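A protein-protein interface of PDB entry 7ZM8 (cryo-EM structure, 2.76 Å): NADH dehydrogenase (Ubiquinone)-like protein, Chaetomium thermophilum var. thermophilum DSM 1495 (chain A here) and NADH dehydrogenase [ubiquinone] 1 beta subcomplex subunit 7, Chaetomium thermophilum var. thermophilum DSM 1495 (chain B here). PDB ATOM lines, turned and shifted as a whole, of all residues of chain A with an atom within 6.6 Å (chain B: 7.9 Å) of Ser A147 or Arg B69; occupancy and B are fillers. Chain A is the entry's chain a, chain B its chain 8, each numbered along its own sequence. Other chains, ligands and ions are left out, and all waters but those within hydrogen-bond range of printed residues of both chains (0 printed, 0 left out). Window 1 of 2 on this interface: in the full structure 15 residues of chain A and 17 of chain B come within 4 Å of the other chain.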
ATOM      1  N   ASP A 144      -0.043  17.549  16.826  1.00  0.00           N
ATOM      2  CA  ASP A 144      -1.216  18.376  17.039  1.00  0.00           C
ATOM      3  C   ASP A 144      -0.945  19.373  18.160  1.00  0.00           C
ATOM      4  O   ASP A 144      -0.054  19.180  18.989  1.00  0.00           O
ATOM      5  CB  ASP A 144      -2.425  17.505  17.379  1.00  0.00           C
ATOM      6  CG  ASP A 144      -3.709  18.299  17.474  1.00  0.00           C
ATOM      7  OD1 ASP A 144      -4.237  18.702  16.418  1.00  0.00           O
ATOM      8  OD2 ASP A 144      -4.188  18.523  18.605  1.00  0.00           O
ATOM      9  N   ARG A 145      -1.716  20.457  18.174  1.00  0.00           N
ATOM     10  CA  ARG A 145      -1.562  21.438  19.236  1.00  0.00           C
ATOM     11  C   ARG A 145      -1.932  20.817  20.576  1.00  0.00           C
ATOM     12  O   ARG A 145      -2.888  20.045  20.681  1.00  0.00           O
ATOM     13  CB  ARG A 145      -2.405  22.683  18.961  1.00  0.00           C
ATOM     14  CG  ARG A 145      -3.896  22.477  19.005  1.00  0.00           C
ATOM     15  CD  ARG A 145      -4.637  23.800  18.935  1.00  0.00           C
ATOM     16  NE  ARG A 145      -4.229  24.704  20.007  1.00  0.00           N
ATOM     17  CZ  ARG A 145      -4.244  26.029  19.916  1.00  0.00           C
ATOM     18  NH1 ARG A 145      -3.851  26.772  20.942  1.00  0.00           N
ATOM     19  NH2 ARG A 145      -4.647  26.616  18.799  1.00  0.00           N
ATOM     20  N   VAL A 146      -1.149  21.144  21.598  1.00  0.00           N
ATOM     21  CA  VAL A 146      -1.230  20.437  22.869  1.00  0.00           C
ATOM     22  C   VAL A 146      -2.068  21.174  23.907  1.00  0.00           C
ATOM     23  O   VAL A 146      -2.541  20.542  24.862  1.00  0.00           O
ATOM     24  CB  VAL A 146       0.185  20.166  23.419  1.00  0.00           C
ATOM     25  CG1 VAL A 146       0.779  21.432  24.005  1.00  0.00           C
ATOM     26  CG2 VAL A 146       0.167  19.031  24.440  1.00  0.00           C
ATOM     27  N   SER A 147      -2.278  22.472  23.745  1.00  0.00           N
ATOM     28  CA  SER A 147      -3.016  23.278  24.702  1.00  0.00           C
ATOM     29  C   SER A 147      -4.175  23.960  23.996  1.00  0.00           C
ATOM     30  O   SER A 147      -4.076  24.303  22.815  1.00  0.00           O
ATOM     31  CB  SER A 147      -2.108  24.319  25.348  1.00  0.00           C
ATOM     32  OG  SER A 147      -2.825  25.124  26.261  1.00  0.00           O
ATOM     33  N   TYR A 148      -5.279  24.127  24.714  1.00  0.00           N
ATOM     34  CA  TYR A 148      -6.436  24.818  24.173  1.00  0.00           C
ATOM     35  C   TYR A 148      -6.109  26.294  23.948  1.00  0.00           C
ATOM     36  O   TYR A 148      -5.315  26.877  24.689  1.00  0.00           O
ATOM     37  CB  TYR A 148      -7.618  24.690  25.132  1.00  0.00           C
ATOM     38  CG  TYR A 148      -8.976  24.789  24.485  1.00  0.00           C
ATOM     39  CD1 TYR A 148      -9.589  23.670  23.950  1.00  0.00           C
ATOM     40  CD2 TYR A 148      -9.643  26.002  24.411  1.00  0.00           C
ATOM     41  CE1 TYR A 148     -10.832  23.754  23.359  1.00  0.00           C
ATOM     42  CE2 TYR A 148     -10.882  26.096  23.822  1.00  0.00           C
ATOM     43  CZ  TYR A 148     -11.474  24.970  23.299  1.00  0.00           C
ATOM     44  OH  TYR A 148     -12.713  25.058  22.709  1.00  0.00           O
ATOM     45  N   PRO A 149      -6.697  26.917  22.927  1.00  0.00           N
ATOM     46  CA  PRO A 149      -6.452  28.347  22.701  1.00  0.00           C
ATOM     47  C   PRO A 149      -6.850  29.181  23.907  1.00  0.00           C
ATOM     48  O   PRO A 149      -7.843  28.905  24.579  1.00  0.00           O
ATOM     49  CB  PRO A 149      -7.318  28.670  21.482  1.00  0.00           C
ATOM     50  CG  PRO A 149      -7.517  27.388  20.798  1.00  0.00           C
ATOM     51  CD  PRO A 149      -7.441  26.297  21.820  1.00  0.00           C
ATOM     52  N   ARG A 150      -6.057  30.215  24.173  1.00  0.00           N
ATOM     53  CA  ARG A 150      -6.219  31.001  25.388  1.00  0.00           C
ATOM     54  C   ARG A 150      -7.416  31.935  25.247  1.00  0.00           C
ATOM     55  O   ARG A 150      -7.609  32.561  24.203  1.00  0.00           O
ATOM     56  CB  ARG A 150      -4.939  31.782  25.670  1.00  0.00           C
ATOM     57  CG  ARG A 150      -4.800  32.251  27.094  1.00  0.00           C
ATOM     58  CD  ARG A 150      -3.405  32.767  27.354  1.00  0.00           C
ATOM     59  NE  ARG A 150      -2.981  33.692  26.314  1.00  0.00           N
ATOM     60  CZ  ARG A 150      -2.499  34.905  26.556  1.00  0.00           C
ATOM     61  NH1 ARG A 150      -2.143  35.685  25.555  1.00  0.00           N
ATOM     62  NH2 ARG A 150      -2.391  35.343  27.799  1.00  0.00           N
ATOM     63  N   GLU A 151      -8.224  32.017  26.296  1.00  0.00           N
ATOM     64  CA  GLU A 151      -9.544  32.633  26.238  1.00  0.00           C
ATOM     65  C   GLU A 151      -9.540  33.954  26.994  1.00  0.00           C
ATOM     66  O   GLU A 151      -9.051  34.026  28.125  1.00  0.00           O
ATOM     67  CB  GLU A 151     -10.589  31.688  26.831  1.00  0.00           C
ATOM     68  CG  GLU A 151     -11.970  32.277  27.018  1.00  0.00           C
ATOM     69  CD  GLU A 151     -12.851  32.066  25.810  1.00  0.00           C
ATOM     70  OE1 GLU A 151     -12.438  31.316  24.900  1.00  0.00           O
ATOM     71  OE2 GLU A 151     -13.963  32.633  25.780  1.00  0.00           O
ATOM     72  N   ASP B  28      -4.951  38.741  30.343  1.00  0.00           N
ATOM     73  CA  ASP B  28      -5.618  37.514  30.717  1.00  0.00           C
ATOM     74  C   ASP B  28      -5.783  37.457  32.234  1.00  0.00           C
ATOM     75  O   ASP B  28      -5.509  38.424  32.944  1.00  0.00           O
ATOM     76  CB  ASP B  28      -4.857  36.322  30.129  1.00  0.00           C
ATOM     77  CG  ASP B  28      -3.439  36.196  30.659  1.00  0.00           C
ATOM     78  OD1 ASP B  28      -2.999  37.048  31.458  1.00  0.00           O
ATOM     79  OD2 ASP B  28      -2.750  35.236  30.256  1.00  0.00           O
ATOM     80  N   GLN B  62       1.065  31.460  35.281  1.00  0.00           N
ATOM     81  CA  GLN B  62       0.857  31.134  33.875  1.00  0.00           C
ATOM     82  C   GLN B  62       0.980  29.644  33.613  1.00  0.00           C
ATOM     83  O   GLN B  62       0.359  29.126  32.679  1.00  0.00           O
ATOM     84  CB  GLN B  62       1.862  31.897  33.016  1.00  0.00           C
ATOM     85  CG  GLN B  62       1.553  33.357  32.843  1.00  0.00           C
ATOM     86  CD  GLN B  62       0.526  33.601  31.764  1.00  0.00           C
ATOM     87  OE1 GLN B  62      -0.488  32.911  31.683  1.00  0.00           O
ATOM     88  NE2 GLN B  62       0.769  34.611  30.941  1.00  0.00           N
ATOM     89  N   TYR B  63       1.782  28.950  34.415  1.00  0.00           N
ATOM     90  CA  TYR B  63       1.934  27.484  34.238  1.00  0.00           C
ATOM     91  C   TYR B  63       0.616  26.804  34.585  1.00  0.00           C
ATOM     92  O   TYR B  63       0.223  25.890  33.857  1.00  0.00           O
ATOM     93  CB  TYR B  63       3.078  26.938  35.090  1.00  0.00           C
ATOM     94  CG  TYR B  63       3.410  25.492  34.827  1.00  0.00           C
ATOM     95  CD1 TYR B  63       3.860  25.079  33.585  1.00  0.00           C
ATOM     96  CD2 TYR B  63       3.275  24.536  35.819  1.00  0.00           C
ATOM     97  CE1 TYR B  63       4.168  23.753  33.333  1.00  0.00           C
ATOM     98  CE2 TYR B  63       3.579  23.206  35.585  1.00  0.00           C
ATOM     99  CZ  TYR B  63       4.029  22.814  34.338  1.00  0.00           C
ATOM    100  OH  TYR B  63       4.329  21.504  34.099  1.00  0.00           O
ATOM    101  N   LEU B  64      -0.051  27.262  35.643  1.00  0.00           N
ATOM    102  CA  LEU B  64      -1.276  26.608  36.093  1.00  0.00           C
ATOM    103  C   LEU B  64      -2.390  26.691  35.056  1.00  0.00           C
ATOM    104  O   LEU B  64      -3.100  25.705  34.832  1.00  0.00           O
ATOM    105  CB  LEU B  64      -1.744  27.199  37.424  1.00  0.00           C
ATOM    106  CG  LEU B  64      -1.135  26.691  38.738  1.00  0.00           C
ATOM    107  CD1 LEU B  64      -1.479  25.222  38.942  1.00  0.00           C
ATOM    108  CD2 LEU B  64       0.364  26.887  38.807  1.00  0.00           C
ATOM    109  N   GLU B  65      -2.583  27.855  34.428  1.00  0.00           N
ATOM    110  CA  GLU B  65      -3.628  27.940  33.413  1.00  0.00           C
ATOM    111  C   GLU B  65      -3.227  27.214  32.140  1.00  0.00           C
ATOM    112  O   GLU B  65      -4.092  26.729  31.401  1.00  0.00           O
ATOM    113  CB  GLU B  65      -4.002  29.389  33.099  1.00  0.00           C
ATOM    114  CG  GLU B  65      -4.822  30.078  34.177  1.00  0.00           C
ATOM    115  CD  GLU B  65      -3.974  30.776  35.197  1.00  0.00           C
ATOM    116  OE1 GLU B  65      -2.754  30.838  34.978  1.00  0.00           O
ATOM    117  OE2 GLU B  65      -4.519  31.258  36.213  1.00  0.00           O
ATOM    118  N   PHE B  66      -1.931  27.131  31.857  1.00  0.00           N
ATOM    119  CA  PHE B  66      -1.497  26.301  30.743  1.00  0.00           C
ATOM    120  C   PHE B  66      -1.856  24.847  30.992  1.00  0.00           C
ATOM    121  O   PHE B  66      -2.361  24.163  30.098  1.00  0.00           O
ATOM    122  CB  PHE B  66       0.008  26.463  30.528  1.00  0.00           C
ATOM    123  CG  PHE B  66       0.596  25.463  29.590  1.00  0.00           C
ATOM    124  CD1 PHE B  66       0.477  25.626  28.223  1.00  0.00           C
ATOM    125  CD2 PHE B  66       1.271  24.364  30.070  1.00  0.00           C
ATOM    126  CE1 PHE B  66       1.022  24.707  27.357  1.00  0.00           C
ATOM    127  CE2 PHE B  66       1.812  23.447  29.212  1.00  0.00           C
ATOM    128  CZ  PHE B  66       1.688  23.617  27.854  1.00  0.00           C
ATOM    129  N   LYS B  67      -1.632  24.368  32.215  1.00  0.00           N
ATOM    130  CA  LYS B  67      -1.979  22.994  32.548  1.00  0.00           C
ATOM    131  C   LYS B  67      -3.479  22.755  32.427  1.00  0.00           C
ATOM    132  O   LYS B  67      -3.908  21.714  31.917  1.00  0.00           O
ATOM    133  CB  LYS B  67      -1.493  22.660  33.956  1.00  0.00           C
ATOM    134  CG  LYS B  67       0.008  22.757  34.130  1.00  0.00           C
ATOM    135  CD  LYS B  67       0.729  21.772  33.229  1.00  0.00           C
ATOM    136  CE  LYS B  67       0.449  20.337  33.646  1.00  0.00           C
ATOM    137  NZ  LYS B  67       0.994  20.033  34.999  1.00  0.00           N
ATOM    138  N   LYS B  68      -4.296  23.703  32.892  1.00  0.00           N
ATOM    139  CA  LYS B  68      -5.737  23.555  32.726  1.00  0.00           C
ATOM    140  C   LYS B  68      -6.139  23.556  31.258  1.00  0.00           C
ATOM    141  O   LYS B  68      -7.065  22.836  30.874  1.00  0.00           O
ATOM    142  CB  LYS B  68      -6.490  24.645  33.488  1.00  0.00           C
ATOM    143  CG  LYS B  68      -6.314  24.587  35.000  1.00  0.00           C
ATOM    144  CD  LYS B  68      -7.152  25.649  35.711  1.00  0.00           C
ATOM    145  CE  LYS B  68      -6.640  27.062  35.499  1.00  0.00           C
ATOM    146  NZ  LYS B  68      -5.313  27.269  36.131  1.00  0.00           N
ATOM    147  N   ARG B  69      -5.469  24.358  30.430  1.00  0.00           N
ATOM    148  CA  ARG B  69      -5.770  24.347  29.004  1.00  0.00           C
ATOM    149  C   ARG B  69      -5.167  23.135  28.310  1.00  0.00           C
ATOM    150  O   ARG B  69      -5.610  22.768  27.216  1.00  0.00           O
ATOM    151  CB  ARG B  69      -5.277  25.632  28.353  1.00  0.00           C
ATOM    152  CG  ARG B  69      -6.044  26.858  28.789  1.00  0.00           C
ATOM    153  CD  ARG B  69      -5.547  28.094  28.079  1.00  0.00           C
ATOM    154  NE  ARG B  69      -4.206  28.457  28.506  1.00  0.00           N
ATOM    155  CZ  ARG B  69      -3.127  28.323  27.746  1.00  0.00           C
ATOM    156  NH1 ARG B  69      -1.939  28.679  28.209  1.00  0.00           N
ATOM    157  NH2 ARG B  69      -3.240  27.829  26.524  1.00  0.00           N
ATOM    158  N   VAL B  70      -4.152  22.517  28.908  1.00  0.00           N
ATOM    159  CA  VAL B  70      -3.633  21.267  28.363  1.00  0.00           C
ATOM    160  C   VAL B  70      -4.631  20.143  28.587  1.00  0.00           C
ATOM    161  O   VAL B  70      -4.942  19.373  27.672  1.00  0.00           O
ATOM    162  CB  VAL B  70      -2.264  20.939  28.980  1.00  0.00           C
ATOM    163  CG1 VAL B  70      -1.929  19.475  28.767  1.00  0.00           C
ATOM    164  CG2 VAL B  70      -1.206  21.806  28.360  1.00  0.00           C
ATOM    165  N   GLN B  71      -5.153  20.038  29.808  1.00  0.00           N
ATOM    166  CA  GLN B  71      -6.151  19.019  30.095  1.00  0.00           C
ATOM    167  C   GLN B  71      -7.432  19.282  29.325  1.00  0.00           C
ATOM    168  O   GLN B  71      -8.151  18.341  28.975  1.00  0.00           O
ATOM    169  CB  GLN B  71      -6.426  18.968  31.597  1.00  0.00           C
ATOM    170  CG  GLN B  71      -7.174  17.728  32.065  1.00  0.00           C
ATOM    171  CD  GLN B  71      -8.677  17.876  31.969  1.00  0.00           C
ATOM    172  OE1 GLN B  71      -9.213  18.977  32.081  1.00  0.00           O
ATOM    173  NE2 GLN B  71      -9.366  16.762  31.758  1.00  0.00           N
ATOM    174  N   LYS B  72      -7.723  20.550  29.036  1.00  0.00           N
ATOM    175  CA  LYS B  72      -8.964  20.895  28.359  1.00  0.00           C
ATOM    176  C   LYS B  72      -8.997  20.412  26.916  1.00  0.00           C
ATOM    177  O   LYS B  72     -10.058  20.464  26.290  1.00  0.00           O
ATOM    178  CB  LYS B  72      -9.193  22.402  28.421  1.00  0.00           C
ATOM    179  N   MET B  73      -7.871  19.953  26.368  1.00  0.00           N
ATOM    180  CA  MET B  73      -7.911  19.242  25.098  1.00  0.00           C
ATOM    181  C   MET B  73      -7.786  17.735  25.236  1.00  0.00           C
ATOM    182  O   MET B  73      -8.152  17.016  24.301  1.00  0.00           O
ATOM    183  CB  MET B  73      -6.815  19.713  24.145  1.00  0.00           C
ATOM    184  CG  MET B  73      -7.154  20.965  23.391  1.00  0.00           C
ATOM    185  SD  MET B  73      -5.785  21.464  22.348  1.00  0.00           S
ATOM    186  CE  MET B  73      -6.524  21.115  20.758  1.00  0.00           C
ATOM    187  N   GLU B  74      -7.272  17.238  26.362  1.00  0.00           N
ATOM    188  CA  GLU B  74      -7.168  15.793  26.525  1.00  0.00           C
ATOM    189  C   GLU B  74      -8.538  15.132  26.471  1.00  0.00           C
ATOM    190  O   GLU B  74      -8.656  13.981  26.036  1.00  0.00           O
ATOM    191  CB  GLU B  74      -6.450  15.459  27.831  1.00  0.00           C
ATOM    192  CG  GLU B  74      -4.938  15.437  27.692  1.00  0.00           C
ATOM    193  CD  GLU B  74      -4.225  15.477  29.027  1.00  0.00           C
ATOM    194  OE1 GLU B  74      -4.859  15.869  30.030  1.00  0.00           O
ATOM    195  OE2 GLU B  74      -3.031  15.113  29.074  1.00  0.00           O
ATOM    196  N   ARG B  77      -9.461  15.763  22.417  1.00  0.00           N
ATOM    197  CA  ARG B  77      -8.814  14.873  21.458  1.00  0.00           C
ATOM    198  C   ARG B  77      -9.465  13.496  21.454  1.00  0.00           C
ATOM    199  O   ARG B  77      -9.693  12.913  20.388  1.00  0.00           O
ATOM    200  CB  ARG B  77      -7.322  14.760  21.768  1.00  0.00           C
ATOM    201  CG  ARG B  77      -6.537  13.989  20.723  1.00  0.00           C
ATOM    202  CD  ARG B  77      -5.044  14.084  20.971  1.00  0.00           C
ATOM    203  NE  ARG B  77      -4.565  15.457  20.863  1.00  0.00           N
ATOM    204  CZ  ARG B  77      -4.069  16.156  21.878  1.00  0.00           C
ATOM    205  NH1 ARG B  77      -3.656  17.401  21.690  1.00  0.00           N
ATOM    206  NH2 ARG B  77      -3.982  15.607  23.081  1.00  0.00           N
ATOM    207  N   SER B  85      -6.505  18.409  15.068  1.00  0.00           N
ATOM    208  CA  SER B  85      -7.251  19.542  15.592  1.00  0.00           C
ATOM    209  C   SER B  85      -6.551  20.880  15.406  1.00  0.00           C
ATOM    210  O   SER B  85      -7.113  21.911  15.792  1.00  0.00           O
ATOM    211  CB  SER B  85      -7.549  19.335  17.083  1.00  0.00           C
ATOM    212  OG  SER B  85      -8.167  20.481  17.640  1.00  0.00           O
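O of Ser A147 lies within hydrogen-bond range of NE of Arg A145 (2.8 Å).
The backbone carbonyl oxygen (O) of Glu B65 lies close to the guanidinium group (NE) of Arg B69, 3.4 Å away.
Printed residues of chain A that touch a printed residue of chain B: Asp A144, Arg A145, Val A146, Ser A147, Tyr A148 and Arg A150.
Along chain A the printed residues that touch a printed residue of chain B span positions 144 to 150.
Printed residues of chain B that touch a printed residue of chain A: Asp B28, Phe B66, Arg B69, Val B70, Lys B72, Met B73, Arg B77 and Ser B85.
Hydrophobic or aromatic side chains of chain B that line the printed part of chain A: Phe B66, Val B70 and Met B73.
Among the printed residues, 13 pairs touch across the chains.
Ser A147 touches just these residues of chain B: Phe B66 (3.7 Å), Arg B69 (2.7 Å), Val B70 (3.9 Å) and Met B73 (3.3 Å).
Of the printed residues of chain A, Arg B69 touches Ser A147 and Tyr A148.
Of the printed residues of chain A, Asp B28 touches Arg A150 (2.5 Å).
Of the printed residues of chain A, Ser B85 touches Asp A144.
Of the printed residues of chain B, Tyr A148 touches Arg B69, Lys B72 and Met B73.
Printed residues of chain B within 4 Å of Arg A145: Met B73 and Arg B77.
Of the printed residues of chain B, Asp A144 touches Arg B77 and Ser B85.
Lys B68 touches none of the printed residues of chain A.
The nearest printed residue of chain A that does not touch Arg B69 is Arg A150 (4.02 Å).
The backbone NH (N) of Tyr A148 lies within hydrogen-bond range of the backbone carbonyl oxygen (O) of Arg B69, 2.9 Å away.
The backbone carbonyl oxygen of Arg A145 lies close to the side-chain sulfur of Met B73 (3.6 Å).
OD2 of Asp B28 is in salt-bridge range of NH2 of Arg A150.
The side-chain carboxylate (OD1) of Asp A144 sits at hydrogen-bond distance from the backbone NH (N) of Ser B85.
The backbone NH (N) of Tyr A148 is in hydrogen-bond range of the side-chain sulfur (SD) of Met B73, at 3.6 Å.
The guanidinium group of Arg B77 sits at hydrogen-bond distance from the backbone carbonyl oxygen of Arg A145.
O of Ser A147 lies close to SD of Met B73 (3.3 Å).
OG of Ser A147 is in hydrogen-bond range of NH2 of Arg B69 (2.7 Å).
OD2 of Asp A144 lies within salt-bridge range of NH1 of Arg B77 (3.3 Å).
Among the printed residues, pairs that only touch across the chains: Val A146 with Val B70 (3.7 Å), Ser A147 with Phe B66 (3.7 Å), Ser A147 with Val B70 (3.9 Å) and Tyr A148 with Lys B72 (3.997 Å).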
